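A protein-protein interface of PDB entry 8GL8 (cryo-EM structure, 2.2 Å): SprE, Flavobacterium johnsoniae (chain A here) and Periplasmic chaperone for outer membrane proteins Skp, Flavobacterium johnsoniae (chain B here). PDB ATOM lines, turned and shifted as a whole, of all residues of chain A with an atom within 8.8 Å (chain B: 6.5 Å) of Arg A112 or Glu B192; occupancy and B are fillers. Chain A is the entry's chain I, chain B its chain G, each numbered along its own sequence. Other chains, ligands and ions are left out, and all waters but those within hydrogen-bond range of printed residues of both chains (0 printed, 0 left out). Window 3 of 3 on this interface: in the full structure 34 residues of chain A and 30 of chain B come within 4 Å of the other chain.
Of the printed residues of chain B, Phe A28 touches Asn B196 (3.98 Å). Of the printed residues of chain B, Arg A31 touches Glu B195. Arg A112 touches one residue of chain B. Printed residues of chain A within 4 Å of Gln B188: Asn A151. Ala B190 touches none of the printed residues of chain A. Printed residues of chain A within 4 Å of Glu B192: Arg A112 (3.8 Å) and Asn A151 (3.2 Å). Arg B194 touches none of the printed residues of chain A. Of the printed residues of chain A, Glu B195 touches Asn A26 and Arg A31. Of the printed residues of chain A, Asn B196 touches Phe A28. The nearest residue of chain A that does not touch Glu B192 is Arg A31 (5.7 Å). The nearest printed residue of chain A that does not touch Gln B188 is Arg A112 (7.2 Å).
Among the printed residues, merely in contact across the chains: Asn A26 with Glu B195, Arg A112 with Glu B192, Asn A151 with Gln B188 and Phe A28 with Asn B196.
The side-chain carboxylate (OE2) of Glu B192 sits at hydrogen-bond distance from the side-chain amide nitrogen (ND2) of Asn A151 (3.2 Å). The side-chain carboxylate of Glu B195 lies within salt-bridge range of the guanidinium group of Arg A31 (2.5 Å).
N of Arg A112 sits at hydrogen-bond distance from OD1 of Asn A108, 3.2 Å away. The backbone carbonyl oxygen (O) of Arg A112 sits at hydrogen-bond distance from the guanidinium group (NE) of Arg A114 (3.0 Å). The side-chain amide nitrogen (ND2) of Asn A26 sits close to the guanidinium group (NH1) of Arg A114 (3.5 Å). NE of Arg A31 lies within hydrogen-bond range of OD1 of Asn A26, at 3.1 Å. The side-chain amino group (NZ) of Lys B191 sits at hydrogen-bond distance from the side-chain amide oxygen (OE1) of Gln B188 (3.2 Å). The side-chain amide oxygen (OD1) of Asn B196 sits close to the side-chain carboxylate (OE1) of Glu B195, at 3.2 Å.
Printed residues of chain B that touch a printed residue of chain A: Gln B188, Glu B192, Glu B195 and Asn B196. Among the printed residues, 6 pairs touch across the chains.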
ATOM      1  N   THR A  23       7.047  28.537  21.331  1.00  0.00           N
ATOM      2  CA  THR A  23       8.356  28.497  21.968  1.00  0.00           C
ATOM      3  C   THR A  23       8.361  29.149  23.344  1.00  0.00           C
ATOM      4  O   THR A  23       9.419  29.230  23.976  1.00  0.00           O
ATOM      5  CB  THR A  23       9.399  29.170  21.075  1.00  0.00           C
ATOM      6  OG1 THR A  23       8.809  30.295  20.411  1.00  0.00           O
ATOM      7  CG2 THR A  23       9.919  28.195  20.035  1.00  0.00           C
ATOM      8  N   ASN A  26       6.737  26.056  28.441  1.00  0.00           N
ATOM      9  CA  ASN A  26       7.640  24.942  28.734  1.00  0.00           C
ATOM     10  C   ASN A  26       6.875  23.645  28.979  1.00  0.00           C
ATOM     11  O   ASN A  26       7.043  22.977  29.998  1.00  0.00           O
ATOM     12  CB  ASN A  26       8.527  25.291  29.922  1.00  0.00           C
ATOM     13  CG  ASN A  26       9.699  24.343  30.072  1.00  0.00           C
ATOM     14  OD1 ASN A  26      10.035  23.604  29.148  1.00  0.00           O
ATOM     15  ND2 ASN A  26      10.330  24.359  31.241  1.00  0.00           N
ATOM     16  N   PHE A  28       6.080  19.688  28.078  1.00  0.00           N
ATOM     17  CA  PHE A  28       6.889  18.557  27.636  1.00  0.00           C
ATOM     18  C   PHE A  28       6.720  18.323  26.140  1.00  0.00           C
ATOM     19  O   PHE A  28       7.706  18.165  25.407  1.00  0.00           O
ATOM     20  CB  PHE A  28       6.511  17.309  28.443  1.00  0.00           C
ATOM     21  CG  PHE A  28       7.174  16.037  27.971  1.00  0.00           C
ATOM     22  CD1 PHE A  28       8.233  15.502  28.680  1.00  0.00           C
ATOM     23  CD2 PHE A  28       6.691  15.337  26.873  1.00  0.00           C
ATOM     24  CE1 PHE A  28       8.839  14.330  28.270  1.00  0.00           C
ATOM     25  CE2 PHE A  28       7.290  14.165  26.459  1.00  0.00           C
ATOM     26  CZ  PHE A  28       8.364  13.658  27.160  1.00  0.00           C
ATOM     27  N   ARG A  31       8.356  21.317  24.043  1.00  0.00           N
ATOM     28  CA  ARG A  31       9.814  21.273  24.024  1.00  0.00           C
ATOM     29  C   ARG A  31      10.321  20.089  23.209  1.00  0.00           C
ATOM     30  O   ARG A  31      11.253  20.232  22.405  1.00  0.00           O
ATOM     31  CB  ARG A  31      10.343  21.215  25.456  1.00  0.00           C
ATOM     32  CG  ARG A  31      11.746  20.662  25.592  1.00  0.00           C
ATOM     33  CD  ARG A  31      12.196  20.704  27.041  1.00  0.00           C
ATOM     34  NE  ARG A  31      11.069  20.893  27.947  1.00  0.00           N
ATOM     35  CZ  ARG A  31      10.565  19.946  28.724  1.00  0.00           C
ATOM     36  NH1 ARG A  31      11.070  18.723  28.741  1.00  0.00           N
ATOM     37  NH2 ARG A  31       9.525  20.230  29.503  1.00  0.00           N
ATOM     38  N   SER A 106      14.446  28.110  19.153  1.00  0.00           N
ATOM     39  CA  SER A 106      15.026  28.350  20.467  1.00  0.00           C
ATOM     40  C   SER A 106      13.916  28.626  21.471  1.00  0.00           C
ATOM     41  O   SER A 106      13.021  29.436  21.212  1.00  0.00           O
ATOM     42  CB  SER A 106      15.998  29.525  20.425  1.00  0.00           C
ATOM     43  OG  SER A 106      16.894  29.488  21.521  1.00  0.00           O
ATOM     44  N   MET A 107      13.975  27.951  22.615  1.00  0.00           N
ATOM     45  CA  MET A 107      12.985  28.110  23.678  1.00  0.00           C
ATOM     46  C   MET A 107      13.705  28.659  24.905  1.00  0.00           C
ATOM     47  O   MET A 107      14.115  27.904  25.790  1.00  0.00           O
ATOM     48  CB  MET A 107      12.293  26.785  23.970  1.00  0.00           C
ATOM     49  CG  MET A 107      11.605  26.178  22.760  1.00  0.00           C
ATOM     50  SD  MET A 107      10.712  24.661  23.138  1.00  0.00           S
ATOM     51  CE  MET A 107       9.950  25.090  24.698  1.00  0.00           C
ATOM     52  N   ASN A 108      13.853  29.983  24.954  1.00  0.00           N
ATOM     53  CA  ASN A 108      14.459  30.668  26.094  1.00  0.00           C
ATOM     54  C   ASN A 108      13.328  31.253  26.935  1.00  0.00           C
ATOM     55  O   ASN A 108      13.014  32.441  26.876  1.00  0.00           O
ATOM     56  CB  ASN A 108      15.437  31.738  25.622  1.00  0.00           C
ATOM     57  CG  ASN A 108      16.555  31.985  26.614  1.00  0.00           C
ATOM     58  OD1 ASN A 108      16.567  31.418  27.706  1.00  0.00           O
ATOM     59  ND2 ASN A 108      17.501  32.835  26.239  1.00  0.00           N
ATOM     60  N   ILE A 109      12.709  30.390  27.735  1.00  0.00           N
ATOM     61  CA  ILE A 109      11.489  30.751  28.450  1.00  0.00           C
ATOM     62  C   ILE A 109      11.795  31.459  29.763  1.00  0.00           C
ATOM     63  O   ILE A 109      11.266  32.541  30.034  1.00  0.00           O
ATOM     64  CB  ILE A 109      10.627  29.490  28.672  1.00  0.00           C
ATOM     65  CG1 ILE A 109       9.882  29.134  27.387  1.00  0.00           C
ATOM     66  CG2 ILE A 109       9.643  29.705  29.811  1.00  0.00           C
ATOM     67  CD1 ILE A 109       9.586  27.665  27.247  1.00  0.00           C
ATOM     68  N   GLY A 110      12.651  30.873  30.595  1.00  0.00           N
ATOM     69  CA  GLY A 110      12.949  31.456  31.889  1.00  0.00           C
ATOM     70  C   GLY A 110      14.414  31.784  32.081  1.00  0.00           C
ATOM     71  O   GLY A 110      14.965  31.584  33.167  1.00  0.00           O
ATOM     72  N   GLY A 111      15.057  32.287  31.031  1.00  0.00           N
ATOM     73  CA  GLY A 111      16.476  32.558  31.068  1.00  0.00           C
ATOM     74  C   GLY A 111      17.355  31.362  30.784  1.00  0.00           C
ATOM     75  O   GLY A 111      18.583  31.515  30.730  1.00  0.00           O
ATOM     76  N   ARG A 112      16.773  30.181  30.600  1.00  0.00           N
ATOM     77  CA  ARG A 112      17.511  28.973  30.269  1.00  0.00           C
ATOM     78  C   ARG A 112      16.895  28.342  29.031  1.00  0.00           C
ATOM     79  O   ARG A 112      15.670  28.308  28.884  1.00  0.00           O
ATOM     80  CB  ARG A 112      17.505  27.974  31.433  1.00  0.00           C
ATOM     81  CG  ARG A 112      18.091  28.528  32.722  1.00  0.00           C
ATOM     82  CD  ARG A 112      17.935  27.559  33.887  1.00  0.00           C
ATOM     83  NE  ARG A 112      17.575  26.214  33.454  1.00  0.00           N
ATOM     84  CZ  ARG A 112      16.405  25.638  33.693  1.00  0.00           C
ATOM     85  NH1 ARG A 112      15.452  26.260  34.369  1.00  0.00           N
ATOM     86  NH2 ARG A 112      16.186  24.404  33.247  1.00  0.00           N
ATOM     87  N   GLU A 113      17.751  27.849  28.140  1.00  0.00           N
ATOM     88  CA  GLU A 113      17.287  27.266  26.889  1.00  0.00           C
ATOM     89  C   GLU A 113      16.638  25.914  27.153  1.00  0.00           C
ATOM     90  O   GLU A 113      17.260  25.021  27.738  1.00  0.00           O
ATOM     91  CB  GLU A 113      18.457  27.125  25.919  1.00  0.00           C
ATOM     92  CG  GLU A 113      18.092  26.515  24.582  1.00  0.00           C
ATOM     93  CD  GLU A 113      17.227  27.426  23.741  1.00  0.00           C
ATOM     94  OE1 GLU A 113      17.448  28.655  23.773  1.00  0.00           O
ATOM     95  OE2 GLU A 113      16.326  26.915  23.047  1.00  0.00           O
ATOM     96  N   ARG A 114      15.384  25.762  26.722  1.00  0.00           N
ATOM     97  CA  ARG A 114      14.678  24.499  26.915  1.00  0.00           C
ATOM     98  C   ARG A 114      15.009  23.498  25.816  1.00  0.00           C
ATOM     99  O   ARG A 114      15.081  22.292  26.073  1.00  0.00           O
ATOM    100  CB  ARG A 114      13.172  24.745  26.976  1.00  0.00           C
ATOM    101  CG  ARG A 114      12.754  25.757  28.025  1.00  0.00           C
ATOM    102  CD  ARG A 114      13.351  25.413  29.376  1.00  0.00           C
ATOM    103  NE  ARG A 114      13.535  26.592  30.211  1.00  0.00           N
ATOM    104  CZ  ARG A 114      13.590  26.569  31.536  1.00  0.00           C
ATOM    105  NH1 ARG A 114      13.475  25.437  32.211  1.00  0.00           N
ATOM    106  NH2 ARG A 114      13.763  27.708  32.198  1.00  0.00           N
ATOM    107  N   ASN A 115      15.205  23.977  24.592  1.00  0.00           N
ATOM    108  CA  ASN A 115      15.603  23.110  23.491  1.00  0.00           C
ATOM    109  C   ASN A 115      17.040  22.649  23.705  1.00  0.00           C
ATOM    110  O   ASN A 115      17.955  23.471  23.798  1.00  0.00           O
ATOM    111  CB  ASN A 115      15.460  23.856  22.167  1.00  0.00           C
ATOM    112  CG  ASN A 115      15.569  22.945  20.965  1.00  0.00           C
ATOM    113  OD1 ASN A 115      15.995  21.798  21.072  1.00  0.00           O
ATOM    114  ND2 ASN A 115      15.183  23.458  19.805  1.00  0.00           N
ATOM    115  N   TYR A 116      17.241  21.337  23.777  1.00  0.00           N
ATOM    116  CA  TYR A 116      18.559  20.780  24.050  1.00  0.00           C
ATOM    117  C   TYR A 116      19.385  20.561  22.790  1.00  0.00           C
ATOM    118  O   TYR A 116      20.501  20.041  22.884  1.00  0.00           O
ATOM    119  CB  TYR A 116      18.435  19.459  24.820  1.00  0.00           C
ATOM    120  CG  TYR A 116      17.303  18.564  24.368  1.00  0.00           C
ATOM    121  CD1 TYR A 116      16.021  18.716  24.882  1.00  0.00           C
ATOM    122  CD2 TYR A 116      17.518  17.562  23.432  1.00  0.00           C
ATOM    123  CE1 TYR A 116      14.987  17.899  24.473  1.00  0.00           C
ATOM    124  CE2 TYR A 116      16.491  16.741  23.017  1.00  0.00           C
ATOM    125  CZ  TYR A 116      15.228  16.912  23.541  1.00  0.00           C
ATOM    126  OH  TYR A 116      14.200  16.095  23.130  1.00  0.00           O
ATOM    127  N   LYS A 148      26.678  30.027  27.096  1.00  0.00           N
ATOM    128  CA  LYS A 148      25.263  29.863  27.390  1.00  0.00           C
ATOM    129  C   LYS A 148      24.873  28.448  27.794  1.00  0.00           C
ATOM    130  O   LYS A 148      23.821  28.272  28.417  1.00  0.00           O
ATOM    131  CB  LYS A 148      24.426  30.282  26.176  1.00  0.00           C
ATOM    132  CG  LYS A 148      23.009  30.701  26.507  1.00  0.00           C
ATOM    133  CD  LYS A 148      22.995  31.872  27.464  1.00  0.00           C
ATOM    134  CE  LYS A 148      21.679  32.620  27.395  1.00  0.00           C
ATOM    135  NZ  LYS A 148      21.758  33.930  28.093  1.00  0.00           N
ATOM    136  N   TYR A 149      25.682  27.443  27.467  1.00  0.00           N
ATOM    137  CA  TYR A 149      25.316  26.040  27.658  1.00  0.00           C
ATOM    138  C   TYR A 149      26.407  25.336  28.453  1.00  0.00           C
ATOM    139  O   TYR A 149      27.295  24.693  27.881  1.00  0.00           O
ATOM    140  CB  TYR A 149      25.072  25.356  26.314  1.00  0.00           C
ATOM    141  CG  TYR A 149      24.124  26.136  25.443  1.00  0.00           C
ATOM    142  CD1 TYR A 149      22.797  26.299  25.809  1.00  0.00           C
ATOM    143  CD2 TYR A 149      24.558  26.737  24.272  1.00  0.00           C
ATOM    144  CE1 TYR A 149      21.927  27.023  25.028  1.00  0.00           C
ATOM    145  CE2 TYR A 149      23.694  27.462  23.485  1.00  0.00           C
ATOM    146  CZ  TYR A 149      22.380  27.602  23.868  1.00  0.00           C
ATOM    147  OH  TYR A 149      21.512  28.326  23.090  1.00  0.00           O
ATOM    148  N   PRO A 150      26.369  25.441  29.780  1.00  0.00           N
ATOM    149  CA  PRO A 150      27.366  24.748  30.606  1.00  0.00           C
ATOM    150  C   PRO A 150      27.101  23.254  30.702  1.00  0.00           C
ATOM    151  O   PRO A 150      28.030  22.463  30.886  1.00  0.00           O
ATOM    152  CB  PRO A 150      27.231  25.429  31.976  1.00  0.00           C
ATOM    153  CG  PRO A 150      26.193  26.515  31.810  1.00  0.00           C
ATOM    154  CD  PRO A 150      25.405  26.191  30.595  1.00  0.00           C
ATOM    155  N   ASN A 151      25.837  22.858  30.578  1.00  0.00           N
ATOM    156  CA  ASN A 151      25.442  21.459  30.657  1.00  0.00           C
ATOM    157  C   ASN A 151      25.512  20.752  29.310  1.00  0.00           C
ATOM    158  O   ASN A 151      25.052  19.612  29.200  1.00  0.00           O
ATOM    159  CB  ASN A 151      24.029  21.339  31.231  1.00  0.00           C
ATOM    160  CG  ASN A 151      23.867  22.079  32.541  1.00  0.00           C
ATOM    161  OD1 ASN A 151      24.730  22.012  33.415  1.00  0.00           O
ATOM    162  ND2 ASN A 151      22.756  22.790  32.686  1.00  0.00           N
ATOM    163  N   SER A 152      26.063  21.401  28.291  1.00  0.00           N
ATOM    164  CA  SER A 152      26.177  20.783  26.981  1.00  0.00           C
ATOM    165  C   SER A 152      27.247  19.697  26.987  1.00  0.00           C
ATOM    166  O   SER A 152      28.164  19.690  27.812  1.00  0.00           O
ATOM    167  CB  SER A 152      26.504  21.835  25.923  1.00  0.00           C
ATOM    168  OG  SER A 152      26.889  21.229  24.703  1.00  0.00           O
ATOM    169  N   GLU B 187      22.574  13.685  36.532  1.00  0.00           N
ATOM    170  CA  GLU B 187      21.963  14.439  37.622  1.00  0.00           C
ATOM    171  C   GLU B 187      21.307  15.715  37.110  1.00  0.00           C
ATOM    172  O   GLU B 187      20.204  16.071  37.540  1.00  0.00           O
ATOM    173  CB  GLU B 187      23.014  14.763  38.685  1.00  0.00           C
ATOM    174  CG  GLU B 187      22.484  15.569  39.859  1.00  0.00           C
ATOM    175  CD  GLU B 187      23.504  16.555  40.392  1.00  0.00           C
ATOM    176  OE1 GLU B 187      24.423  16.127  41.123  1.00  0.00           O
ATOM    177  OE2 GLU B 187      23.388  17.759  40.080  1.00  0.00           O
ATOM    178  N   GLN B 188      21.970  16.416  36.187  1.00  0.00           N
ATOM    179  CA  GLN B 188      21.397  17.631  35.618  1.00  0.00           C
ATOM    180  C   GLN B 188      20.129  17.328  34.830  1.00  0.00           C
ATOM    181  O   GLN B 188      19.150  18.078  34.908  1.00  0.00           O
ATOM    182  CB  GLN B 188      22.424  18.331  34.731  1.00  0.00           C
ATOM    183  CG  GLN B 188      23.529  19.040  35.495  1.00  0.00           C
ATOM    184  CD  GLN B 188      22.999  20.081  36.460  1.00  0.00           C
ATOM    185  OE1 GLN B 188      23.456  20.177  37.599  1.00  0.00           O
ATOM    186  NE2 GLN B 188      22.033  20.872  36.008  1.00  0.00           N
ATOM    187  N   GLU B 189      20.135  16.239  34.056  1.00  0.00           N
ATOM    188  CA  GLU B 189      18.939  15.860  33.311  1.00  0.00           C
ATOM    189  C   GLU B 189      17.788  15.528  34.252  1.00  0.00           C
ATOM    190  O   GLU B 189      16.647  15.948  34.023  1.00  0.00           O
ATOM    191  CB  GLU B 189      19.244  14.675  32.396  1.00  0.00           C
ATOM    192  CG  GLU B 189      18.217  14.458  31.295  1.00  0.00           C
ATOM    193  CD  GLU B 189      17.390  13.205  31.508  1.00  0.00           C
ATOM    194  OE1 GLU B 189      17.398  12.670  32.637  1.00  0.00           O
ATOM    195  OE2 GLU B 189      16.732  12.753  30.547  1.00  0.00           O
ATOM    196  N   ALA B 190      18.071  14.784  35.324  1.00  0.00           N
ATOM    197  CA  ALA B 190      17.030  14.456  36.293  1.00  0.00           C
ATOM    198  C   ALA B 190      16.493  15.709  36.973  1.00  0.00           C
ATOM    199  O   ALA B 190      15.284  15.830  37.203  1.00  0.00           O
ATOM    200  CB  ALA B 190      17.569  13.470  37.330  1.00  0.00           C
ATOM    201  N   LYS B 191      17.378  16.650  37.308  1.00  0.00           N
ATOM    202  CA  LYS B 191      16.944  17.880  37.965  1.00  0.00           C
ATOM    203  C   LYS B 191      16.086  18.735  37.040  1.00  0.00           C
ATOM    204  O   LYS B 191      15.035  19.240  37.451  1.00  0.00           O
ATOM    205  CB  LYS B 191      18.160  18.668  38.448  1.00  0.00           C
ATOM    206  CG  LYS B 191      18.814  18.100  39.699  1.00  0.00           C
ATOM    207  CD  LYS B 191      20.186  18.714  39.941  1.00  0.00           C
ATOM    208  CE  LYS B 191      20.205  20.200  39.614  1.00  0.00           C
ATOM    209  NZ  LYS B 191      21.465  20.851  40.063  1.00  0.00           N
ATOM    210  N   GLU B 192      16.515  18.911  35.788  1.00  0.00           N
ATOM    211  CA  GLU B 192      15.789  19.777  34.866  1.00  0.00           C
ATOM    212  C   GLU B 192      14.547  19.111  34.289  1.00  0.00           C
ATOM    213  O   GLU B 192      13.691  19.807  33.733  1.00  0.00           O
ATOM    214  CB  GLU B 192      16.709  20.230  33.732  1.00  0.00           C
ATOM    215  CG  GLU B 192      17.856  21.121  34.180  1.00  0.00           C
ATOM    216  CD  GLU B 192      18.925  21.275  33.116  1.00  0.00           C
ATOM    217  OE1 GLU B 192      19.042  20.379  32.254  1.00  0.00           O
ATOM    218  OE2 GLU B 192      19.648  22.293  33.140  1.00  0.00           O
ATOM    219  N   ASN B 193      14.429  17.790  34.400  1.00  0.00           N
ATOM    220  CA  ASN B 193      13.257  17.077  33.910  1.00  0.00           C
ATOM    221  C   ASN B 193      12.178  16.911  34.971  1.00  0.00           C
ATOM    222  O   ASN B 193      11.170  16.246  34.709  1.00  0.00           O
ATOM    223  CB  ASN B 193      13.663  15.703  33.369  1.00  0.00           C
ATOM    224  CG  ASN B 193      13.683  15.654  31.854  1.00  0.00           C
ATOM    225  OD1 ASN B 193      13.730  16.689  31.188  1.00  0.00           O
ATOM    226  ND2 ASN B 193      13.647  14.448  31.300  1.00  0.00           N
ATOM    227  N   ARG B 194      12.362  17.494  36.153  1.00  0.00           N
ATOM    228  CA  ARG B 194      11.426  17.334  37.257  1.00  0.00           C
ATOM    229  C   ARG B 194      10.148  18.146  37.084  1.00  0.00           C
ATOM    230  O   ARG B 194       9.188  17.924  37.829  1.00  0.00           O
ATOM    231  CB  ARG B 194      12.107  17.715  38.576  1.00  0.00           C
ATOM    232  CG  ARG B 194      12.578  16.521  39.389  1.00  0.00           C
ATOM    233  CD  ARG B 194      12.803  16.896  40.843  1.00  0.00           C
ATOM    234  NE  ARG B 194      14.206  17.184  41.116  1.00  0.00           N
ATOM    235  CZ  ARG B 194      14.702  18.402  41.288  1.00  0.00           C
ATOM    236  NH1 ARG B 194      13.933  19.476  41.222  1.00  0.00           N
ATOM    237  NH2 ARG B 194      16.001  18.545  41.533  1.00  0.00           N
ATOM    238  N   GLU B 195      10.109  19.074  36.126  1.00  0.00           N
ATOM    239  CA  GLU B 195       8.883  19.823  35.874  1.00  0.00           C
ATOM    240  C   GLU B 195       7.833  18.985  35.157  1.00  0.00           C
ATOM    241  O   GLU B 195       6.636  19.268  35.288  1.00  0.00           O
ATOM    242  CB  GLU B 195       9.191  21.083  35.063  1.00  0.00           C
ATOM    243  CG  GLU B 195      10.227  20.884  33.971  1.00  0.00           C
ATOM    244  CD  GLU B 195       9.616  20.411  32.668  1.00  0.00           C
ATOM    245  OE1 GLU B 195       8.404  20.632  32.463  1.00  0.00           O
ATOM    246  OE2 GLU B 195      10.347  19.817  31.846  1.00  0.00           O
ATOM    247  N   ASN B 196       8.248  17.966  34.410  1.00  0.00           N
ATOM    248  CA  ASN B 196       7.318  17.079  33.720  1.00  0.00           C
ATOM    249  C   ASN B 196       7.944  15.708  33.486  1.00  0.00           C
ATOM    250  O   ASN B 196       8.335  15.023  34.432  1.00  0.00           O
ATOM    251  CB  ASN B 196       6.875  17.688  32.389  1.00  0.00           C
ATOM    252  CG  ASN B 196       5.559  18.433  32.497  1.00  0.00           C
ATOM    253  OD1 ASN B 196       5.449  19.585  32.078  1.00  0.00           O
ATOM    254  ND2 ASN B 196       4.553  17.776  33.060  1.00  0.00           N
